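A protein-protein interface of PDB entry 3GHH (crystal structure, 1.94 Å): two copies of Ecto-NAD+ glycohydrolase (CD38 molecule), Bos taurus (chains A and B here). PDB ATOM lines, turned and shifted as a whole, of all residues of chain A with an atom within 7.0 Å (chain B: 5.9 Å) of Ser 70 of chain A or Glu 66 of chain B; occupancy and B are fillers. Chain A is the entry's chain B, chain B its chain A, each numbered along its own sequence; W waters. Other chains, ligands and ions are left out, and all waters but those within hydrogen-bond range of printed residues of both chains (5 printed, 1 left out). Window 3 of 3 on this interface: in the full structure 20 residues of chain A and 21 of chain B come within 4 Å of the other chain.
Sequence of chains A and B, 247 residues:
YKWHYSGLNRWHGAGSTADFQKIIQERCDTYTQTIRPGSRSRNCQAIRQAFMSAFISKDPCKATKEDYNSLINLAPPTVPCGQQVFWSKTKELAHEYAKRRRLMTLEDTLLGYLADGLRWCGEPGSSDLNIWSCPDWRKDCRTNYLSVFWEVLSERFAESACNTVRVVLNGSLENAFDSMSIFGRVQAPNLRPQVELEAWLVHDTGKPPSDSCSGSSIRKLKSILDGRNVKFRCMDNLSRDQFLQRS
The side-chain amide nitrogen of Asn 69 of chain A lies close to the side-chain amide oxygen of Asn 69 of chain B (3.3 Å). The side-chain amide nitrogen (ND2) of Asn 69 of chain B lies close to the side-chain amide nitrogen (ND2) of Asn 73 of chain A (2.9 Å). The side-chain carboxylate of Glu 66 of chain A sits at hydrogen-bond distance from the side-chain hydroxyl of Ser 70 of chain B, 2.8 Å away. OD1 of Asn 69 of chain A sits close to O of Glu 66 of chain B (3.3 Å). The side-chain amide nitrogen (ND2) of Asn 73 of chain A is in hydrogen-bond range of the side-chain carboxylate (OE2) of Glu 66 of chain B (2.8 Å).
CG of Glu 66 of chain B touches OG of Ser 70 of chain A, 3.4 Å away. OD1 of Asn 69 of chain B touches CG2 of Ile 72 of chain A (3.9 Å). Asn 73 of chain A touches Lys 65 of chain B.
Water W4 bridges the backbone carbonyl oxygen (O) of Ser 70 of chain A (2.8 Å) and the side-chain carboxylate (OE2) of Glu 66 of chain B (3.1 Å). Water W2 lies within hydrogen-bond range of the backbone carbonyl oxygen of Glu 66 of chain B (2.8 Å), the backbone NH of Ser 70 of chain B (2.9 Å), the side-chain amide oxygen of Asn 69 of chain A (3.2 Å) and the backbone NH of Asn 69 of chain B (3.2 Å). Water W1 bridges the side-chain amide oxygen (OD1) of Asn 69 of chain A (2.8 Å) and the backbone carbonyl oxygen (O) of Glu 66 of chain B (3.2 Å). Water W5 bridges ND2 of Asn 69 of chain A and OG of Ser 70 of chain B. Water W3 bridges the side-chain carboxylate of Glu 66 of chain A (3.2 Å) and the side-chain hydroxyl of Ser 70 of chain B (3.2 Å).
O of Lys 65 of chain B is in hydrogen-bond range of ND2 of Asn 69 of chain B. The side-chain amide oxygen (OD1) of Asn 69 of chain A lies close to the backbone carbonyl oxygen (O) of Glu 66 of chain A, at 3.4 Å. The side-chain hydroxyl (OG1) of Thr 64 of chain B lies close to the backbone NH (N) of Glu 66 of chain B (3.5 Å). The backbone carbonyl oxygen (O) of Asn 69 of chain A lies close to the side-chain amide nitrogen (ND2) of Asn 73 of chain A, at 3.4 Å.
Phe 51 of chain A touches none of the printed residues of chain B. Tyr 68 of chain A touches none of the printed residues of chain B. Printed residues of chain B within 4 Å of Asn 69 of chain A: Glu 66 (3.3 Å) and Asn 69 (3.1 Å). Ser 70 of chain A touches one residue of chain B. Of the printed residues of chain B, Ile 72 of chain A touches Asn 69. Of chain A, only Asn 69 (3.3 Å), Ser 70 (3.4 Å) and Asn 73 (2.8 Å) come within 4 Å of Glu 66 of chain B. Of the printed residues of chain A, Ser 70 of chain B touches Glu 66. The nearest residue of chain B that does not touch Ser 70 of chain A is Asn 69 of chain B (5.8 Å). The nearest residue of chain A that does not touch Glu 66 of chain B is Leu 71 of chain A (5.9 Å).
Of the 13 printed residues of chain A, 5 touch a printed residue of chain B. Among the printed residues, 8 pairs touch across the chains. Among the printed residues, no Asp or Glu carboxylate lies within 4 Å of a Lys or Arg side-chain nitrogen of the other chain.
Glu 66 of chain A touches Ser 70 of chain B, and with the chains exchanged Ser 70 of chain A touches Glu 66 of chain B. Asn 69 of chain A touches Glu 66 of chain B, but with the chains exchanged Glu 66 of chain A does not touch Asn 69 of chain B (6.3 Å). Asn 69 of chain B touches its own counterpart, Asn 69 of chain A. Of the 8 pairs that touch across the chains among the printed residues, 3 have their exchanged pair printed and touching as well.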
ATOM      1  N   ALA A  50      12.086 -20.684 -22.616  1.00  0.00           N
ATOM      2  CA  ALA A  50      13.134 -20.774 -23.625  1.00  0.00           C
ATOM      3  C   ALA A  50      12.709 -21.670 -24.782  1.00  0.00           C
ATOM      4  O   ALA A  50      13.017 -21.398 -25.940  1.00  0.00           O
ATOM      5  CB  ALA A  50      14.435 -21.291 -23.009  1.00  0.00           C
ATOM      6  N   PHE A  51      12.028 -22.755 -24.452  1.00  0.00           N
ATOM      7  CA  PHE A  51      11.465 -23.658 -25.456  1.00  0.00           C
ATOM      8  C   PHE A  51      10.488 -22.878 -26.350  1.00  0.00           C
ATOM      9  O   PHE A  51      10.587 -22.902 -27.577  1.00  0.00           O
ATOM     10  CB  PHE A  51      10.724 -24.804 -24.756  1.00  0.00           C
ATOM     11  CG  PHE A  51      10.728 -26.092 -25.522  1.00  0.00           C
ATOM     12  CD1 PHE A  51      10.867 -27.296 -24.865  1.00  0.00           C
ATOM     13  CD2 PHE A  51      10.622 -26.101 -26.898  1.00  0.00           C
ATOM     14  CE1 PHE A  51      10.871 -28.498 -25.567  1.00  0.00           C
ATOM     15  CE2 PHE A  51      10.634 -27.297 -27.605  1.00  0.00           C
ATOM     16  CZ  PHE A  51      10.755 -28.494 -26.935  1.00  0.00           C
ATOM     17  N   LYS A  65      19.637 -24.381 -36.035  1.00  0.00           N
ATOM     18  CA  LYS A  65      20.109 -24.959 -34.784  1.00  0.00           C
ATOM     19  C   LYS A  65      20.295 -23.854 -33.746  1.00  0.00           C
ATOM     20  O   LYS A  65      20.025 -24.051 -32.555  1.00  0.00           O
ATOM     21  CB  LYS A  65      21.413 -25.738 -35.005  1.00  0.00           C
ATOM     22  CG  LYS A  65      21.270 -26.901 -35.990  1.00  0.00           C
ATOM     23  CD  LYS A  65      22.504 -27.797 -36.006  1.00  0.00           C
ATOM     24  CE  LYS A  65      22.299 -29.019 -36.892  1.00  0.00           C
ATOM     25  NZ  LYS A  65      23.434 -29.985 -36.780  1.00  0.00           N
ATOM     26  N   GLU A  66      20.718 -22.684 -34.212  1.00  0.00           N
ATOM     27  CA  GLU A  66      21.011 -21.578 -33.314  1.00  0.00           C
ATOM     28  C   GLU A  66      19.780 -21.191 -32.492  1.00  0.00           C
ATOM     29  O   GLU A  66      19.924 -20.736 -31.365  1.00  0.00           O
ATOM     30  CB  GLU A  66      21.552 -20.361 -34.069  1.00  0.00           C
ATOM     31  CG  GLU A  66      23.005 -20.497 -34.532  1.00  0.00           C
ATOM     32  CD  GLU A  66      23.155 -21.350 -35.781  1.00  0.00           C
ATOM     33  OE1 GLU A  66      22.125 -21.686 -36.402  1.00  0.00           O
ATOM     34  OE2 GLU A  66      24.307 -21.679 -36.148  1.00  0.00           O
ATOM     35  N   ASP A  67      18.585 -21.392 -33.054  1.00  0.00           N
ATOM     36  CA  ASP A  67      17.340 -21.012 -32.375  1.00  0.00           C
ATOM     37  C   ASP A  67      17.175 -21.754 -31.050  1.00  0.00           C
ATOM     38  O   ASP A  67      16.459 -21.302 -30.163  1.00  0.00           O
ATOM     39  CB  ASP A  67      16.115 -21.291 -33.259  1.00  0.00           C
ATOM     40  CG  ASP A  67      15.995 -20.314 -34.416  1.00  0.00           C
ATOM     41  OD1 ASP A  67      16.360 -19.136 -34.234  1.00  0.00           O
ATOM     42  OD2 ASP A  67      15.542 -20.732 -35.500  1.00  0.00           O
ATOM     43  N   TYR A  68      17.821 -22.909 -30.939  1.00  0.00           N
ATOM     44  CA  TYR A  68      17.726 -23.725 -29.733  1.00  0.00           C
ATOM     45  C   TYR A  68      18.902 -23.584 -28.750  1.00  0.00           C
ATOM     46  O   TYR A  68      18.999 -24.361 -27.793  1.00  0.00           O
ATOM     47  CB  TYR A  68      17.543 -25.193 -30.119  1.00  0.00           C
ATOM     48  CG  TYR A  68      16.152 -25.512 -30.624  1.00  0.00           C
ATOM     49  CD1 TYR A  68      15.059 -25.514 -29.758  1.00  0.00           C
ATOM     50  CD2 TYR A  68      15.936 -25.833 -31.958  1.00  0.00           C
ATOM     51  CE1 TYR A  68      13.791 -25.819 -30.210  1.00  0.00           C
ATOM     52  CE2 TYR A  68      14.674 -26.145 -32.419  1.00  0.00           C
ATOM     53  CZ  TYR A  68      13.604 -26.131 -31.544  1.00  0.00           C
ATOM     54  OH  TYR A  68      12.350 -26.441 -32.008  1.00  0.00           O
ATOM     55  N   ASN A  69      19.782 -22.609 -28.987  1.00  0.00           N
ATOM     56  CA  ASN A  69      20.967 -22.394 -28.146  1.00  0.00           C
ATOM     57  C   ASN A  69      20.611 -22.184 -26.669  1.00  0.00           C
ATOM     58  O   ASN A  69      21.155 -22.843 -25.788  1.00  0.00           O
ATOM     59  CB  ASN A  69      21.776 -21.176 -28.629  1.00  0.00           C
ATOM     60  CG  ASN A  69      22.688 -21.482 -29.826  1.00  0.00           C
ATOM     61  OD1 ASN A  69      23.160 -20.567 -30.502  1.00  0.00           O
ATOM     62  ND2 ASN A  69      22.930 -22.752 -30.089  1.00  0.00           N
ATOM     63  N   SER A  70      19.723 -21.234 -26.405  1.00  0.00           N
ATOM     64  CA  SER A  70      19.322 -20.944 -25.030  1.00  0.00           C
ATOM     65  C   SER A  70      18.768 -22.189 -24.334  1.00  0.00           C
ATOM     66  O   SER A  70      19.162 -22.514 -23.204  1.00  0.00           O
ATOM     67  CB  SER A  70      18.309 -19.792 -24.999  1.00  0.00           C
ATOM     68  OG  SER A  70      18.925 -18.583 -25.445  1.00  0.00           O
ATOM     69  N   LEU A  71      17.862 -22.886 -25.015  1.00  0.00           N
ATOM     70  CA  LEU A  71      17.231 -24.087 -24.472  1.00  0.00           C
ATOM     71  C   LEU A  71      18.226 -25.187 -24.116  1.00  0.00           C
ATOM     72  O   LEU A  71      18.193 -25.724 -23.002  1.00  0.00           O
ATOM     73  CB  LEU A  71      16.169 -24.631 -25.437  1.00  0.00           C
ATOM     74  CG  LEU A  71      15.377 -25.867 -24.988  1.00  0.00           C
ATOM     75  CD1 LEU A  71      14.585 -25.578 -23.707  1.00  0.00           C
ATOM     76  CD2 LEU A  71      14.436 -26.323 -26.072  1.00  0.00           C
ATOM     77  N   ILE A  72      19.108 -25.538 -25.051  1.00  0.00           N
ATOM     78  CA  ILE A  72      20.053 -26.613 -24.784  1.00  0.00           C
ATOM     79  C   ILE A  72      21.023 -26.189 -23.677  1.00  0.00           C
ATOM     80  O   ILE A  72      21.441 -27.009 -22.870  1.00  0.00           O
ATOM     81  CB  ILE A  72      20.835 -27.052 -26.038  1.00  0.00           C
ATOM     82  CG1 ILE A  72      21.639 -28.318 -25.738  1.00  0.00           C
ATOM     83  CG2 ILE A  72      21.748 -25.940 -26.523  1.00  0.00           C
ATOM     84  CD1 ILE A  72      22.245 -28.962 -26.979  1.00  0.00           C
ATOM     85  N   ASN A  73      21.360 -24.904 -23.622  1.00  0.00           N
ATOM     86  CA  ASN A  73      22.279 -24.433 -22.594  1.00  0.00           C
ATOM     87  C   ASN A  73      21.679 -24.560 -21.198  1.00  0.00           C
ATOM     88  O   ASN A  73      22.409 -24.736 -20.226  1.00  0.00           O
ATOM     89  CB  ASN A  73      22.728 -22.987 -22.866  1.00  0.00           C
ATOM     90  CG  ASN A  73      23.736 -22.894 -24.001  1.00  0.00           C
ATOM     91  OD1 ASN A  73      24.212 -23.910 -24.491  1.00  0.00           O
ATOM     92  ND2 ASN A  73      24.059 -21.672 -24.425  1.00  0.00           N
ATOM     93  N   LEU A  74      20.349 -24.469 -21.112  1.00  0.00           N
ATOM     94  CA  LEU A  74      19.622 -24.635 -19.852  1.00  0.00           C
ATOM     95  C   LEU A  74      19.583 -26.082 -19.372  1.00  0.00           C
ATOM     96  O   LEU A  74      19.453 -26.345 -18.175  1.00  0.00           O
ATOM     97  CB  LEU A  74      18.194 -24.113 -20.009  1.00  0.00           C
ATOM     98  CG  LEU A  74      17.758 -22.769 -19.420  1.00  0.00           C
ATOM     99  CD1 LEU A  74      18.910 -21.920 -18.893  1.00  0.00           C
ATOM    100  CD2 LEU A  74      16.892 -21.996 -20.405  1.00  0.00           C
ATOM    101  N   ALA A  75      19.672 -27.026 -20.300  1.00  0.00           N
ATOM    102  CA  ALA A  75      19.561 -28.436 -19.939  1.00  0.00           C
ATOM    103  C   ALA A  75      20.226 -29.343 -20.965  1.00  0.00           C
ATOM    104  O   ALA A  75      19.535 -30.010 -21.731  1.00  0.00           O
ATOM    105  CB  ALA A  75      18.086 -28.812 -19.786  1.00  0.00           C
ATOM    106  N   THR B  64      26.847 -13.411 -24.464  1.00  0.00           N
ATOM    107  CA  THR B  64      26.103 -14.462 -23.802  1.00  0.00           C
ATOM    108  C   THR B  64      26.730 -15.794 -24.175  1.00  0.00           C
ATOM    109  O   THR B  64      27.474 -15.908 -25.161  1.00  0.00           O
ATOM    110  CB  THR B  64      24.611 -14.474 -24.200  1.00  0.00           C
ATOM    111  OG1 THR B  64      24.497 -14.754 -25.595  1.00  0.00           O
ATOM    112  CG2 THR B  64      23.946 -13.128 -23.901  1.00  0.00           C
ATOM    113  N   LYS B  65      26.432 -16.804 -23.377  1.00  0.00           N
ATOM    114  CA  LYS B  65      26.889 -18.147 -23.681  1.00  0.00           C
ATOM    115  C   LYS B  65      26.435 -18.553 -25.079  1.00  0.00           C
ATOM    116  O   LYS B  65      27.159 -19.235 -25.801  1.00  0.00           O
ATOM    117  CB  LYS B  65      26.338 -19.137 -22.652  1.00  0.00           C
ATOM    118  CG  LYS B  65      26.896 -18.958 -21.237  1.00  0.00           C
ATOM    119  CD  LYS B  65      26.249 -19.971 -20.279  1.00  0.00           C
ATOM    120  CE  LYS B  65      26.275 -21.379 -20.876  1.00  0.00           C
ATOM    121  NZ  LYS B  65      25.498 -22.382 -20.079  1.00  0.00           N
ATOM    122  N   GLU B  66      25.227 -18.143 -25.453  1.00  0.00           N
ATOM    123  CA  GLU B  66      24.646 -18.579 -26.722  1.00  0.00           C
ATOM    124  C   GLU B  66      25.405 -18.057 -27.952  1.00  0.00           C
ATOM    125  O   GLU B  66      25.326 -18.638 -29.035  1.00  0.00           O
ATOM    126  CB  GLU B  66      23.164 -18.196 -26.803  1.00  0.00           C
ATOM    127  CG  GLU B  66      22.249 -18.972 -25.836  1.00  0.00           C
ATOM    128  CD  GLU B  66      22.465 -18.583 -24.390  1.00  0.00           C
ATOM    129  OE1 GLU B  66      22.486 -17.368 -24.103  1.00  0.00           O
ATOM    130  OE2 GLU B  66      22.632 -19.490 -23.542  1.00  0.00           O
ATOM    131  N   ASP B  67      26.133 -16.960 -27.793  1.00  0.00           N
ATOM    132  CA  ASP B  67      26.943 -16.440 -28.892  1.00  0.00           C
ATOM    133  C   ASP B  67      28.042 -17.420 -29.315  1.00  0.00           C
ATOM    134  O   ASP B  67      28.532 -17.367 -30.438  1.00  0.00           O
ATOM    135  CB  ASP B  67      27.588 -15.115 -28.495  1.00  0.00           C
ATOM    136  CG  ASP B  67      26.585 -13.993 -28.390  1.00  0.00           C
ATOM    137  OD1 ASP B  67      25.595 -14.011 -29.137  1.00  0.00           O
ATOM    138  OD2 ASP B  67      26.797 -13.086 -27.567  1.00  0.00           O
ATOM    139  N   TYR B  68      28.437 -18.311 -28.417  1.00  0.00           N
ATOM    140  CA  TYR B  68      29.551 -19.222 -28.711  1.00  0.00           C
ATOM    141  C   TYR B  68      29.158 -20.653 -29.095  1.00  0.00           C
ATOM    142  O   TYR B  68      30.035 -21.453 -29.435  1.00  0.00           O
ATOM    143  CB  TYR B  68      30.547 -19.258 -27.544  1.00  0.00           C
ATOM    144  CG  TYR B  68      31.451 -18.048 -27.456  1.00  0.00           C
ATOM    145  CD1 TYR B  68      31.338 -17.132 -26.414  1.00  0.00           C
ATOM    146  CD2 TYR B  68      32.425 -17.822 -28.415  1.00  0.00           C
ATOM    147  CE1 TYR B  68      32.180 -16.017 -26.336  1.00  0.00           C
ATOM    148  CE2 TYR B  68      33.259 -16.718 -28.351  1.00  0.00           C
ATOM    149  CZ  TYR B  68      33.144 -15.823 -27.312  1.00  0.00           C
ATOM    150  OH  TYR B  68      34.000 -14.736 -27.250  1.00  0.00           O
ATOM    151  N   ASN B  69      27.863 -20.972 -29.061  1.00  0.00           N
ATOM    152  CA  ASN B  69      27.418 -22.348 -29.290  1.00  0.00           C
ATOM    153  C   ASN B  69      27.924 -22.896 -30.616  1.00  0.00           C
ATOM    154  O   ASN B  69      28.396 -24.024 -30.689  1.00  0.00           O
ATOM    155  CB  ASN B  69      25.883 -22.471 -29.242  1.00  0.00           C
ATOM    156  CG  ASN B  69      25.344 -22.707 -27.833  1.00  0.00           C
ATOM    157  OD1 ASN B  69      24.785 -23.767 -27.534  1.00  0.00           O
ATOM    158  ND2 ASN B  69      25.504 -21.723 -26.969  1.00  0.00           N
ATOM    159  N   SER B  70      27.784 -22.106 -31.674  1.00  0.00           N
ATOM    160  CA  SER B  70      28.202 -22.546 -33.002  1.00  0.00           C
ATOM    161  C   SER B  70      29.705 -22.828 -33.091  1.00  0.00           C
ATOM    162  O   SER B  70      30.120 -23.837 -33.656  1.00  0.00           O
ATOM    163  CB  SER B  70      27.796 -21.521 -34.058  1.00  0.00           C
ATOM    164  OG  SER B  70      26.420 -21.644 -34.354  1.00  0.00           O
HETATM  165  O   HOH W   1      22.506 -17.860 -30.279  1.00  0.00           O
HETATM  166  O   HOH W   2      26.071 -19.786 -31.431  1.00  0.00           O
HETATM  167  O   HOH W   3      26.345 -19.286 -36.505  1.00  0.00           O
HETATM  168  O   HOH W   4      20.234 -20.392 -21.809  1.00  0.00           O
HETATM  169  O   HOH W   5      24.574 -23.618 -32.420  1.00  0.00           O
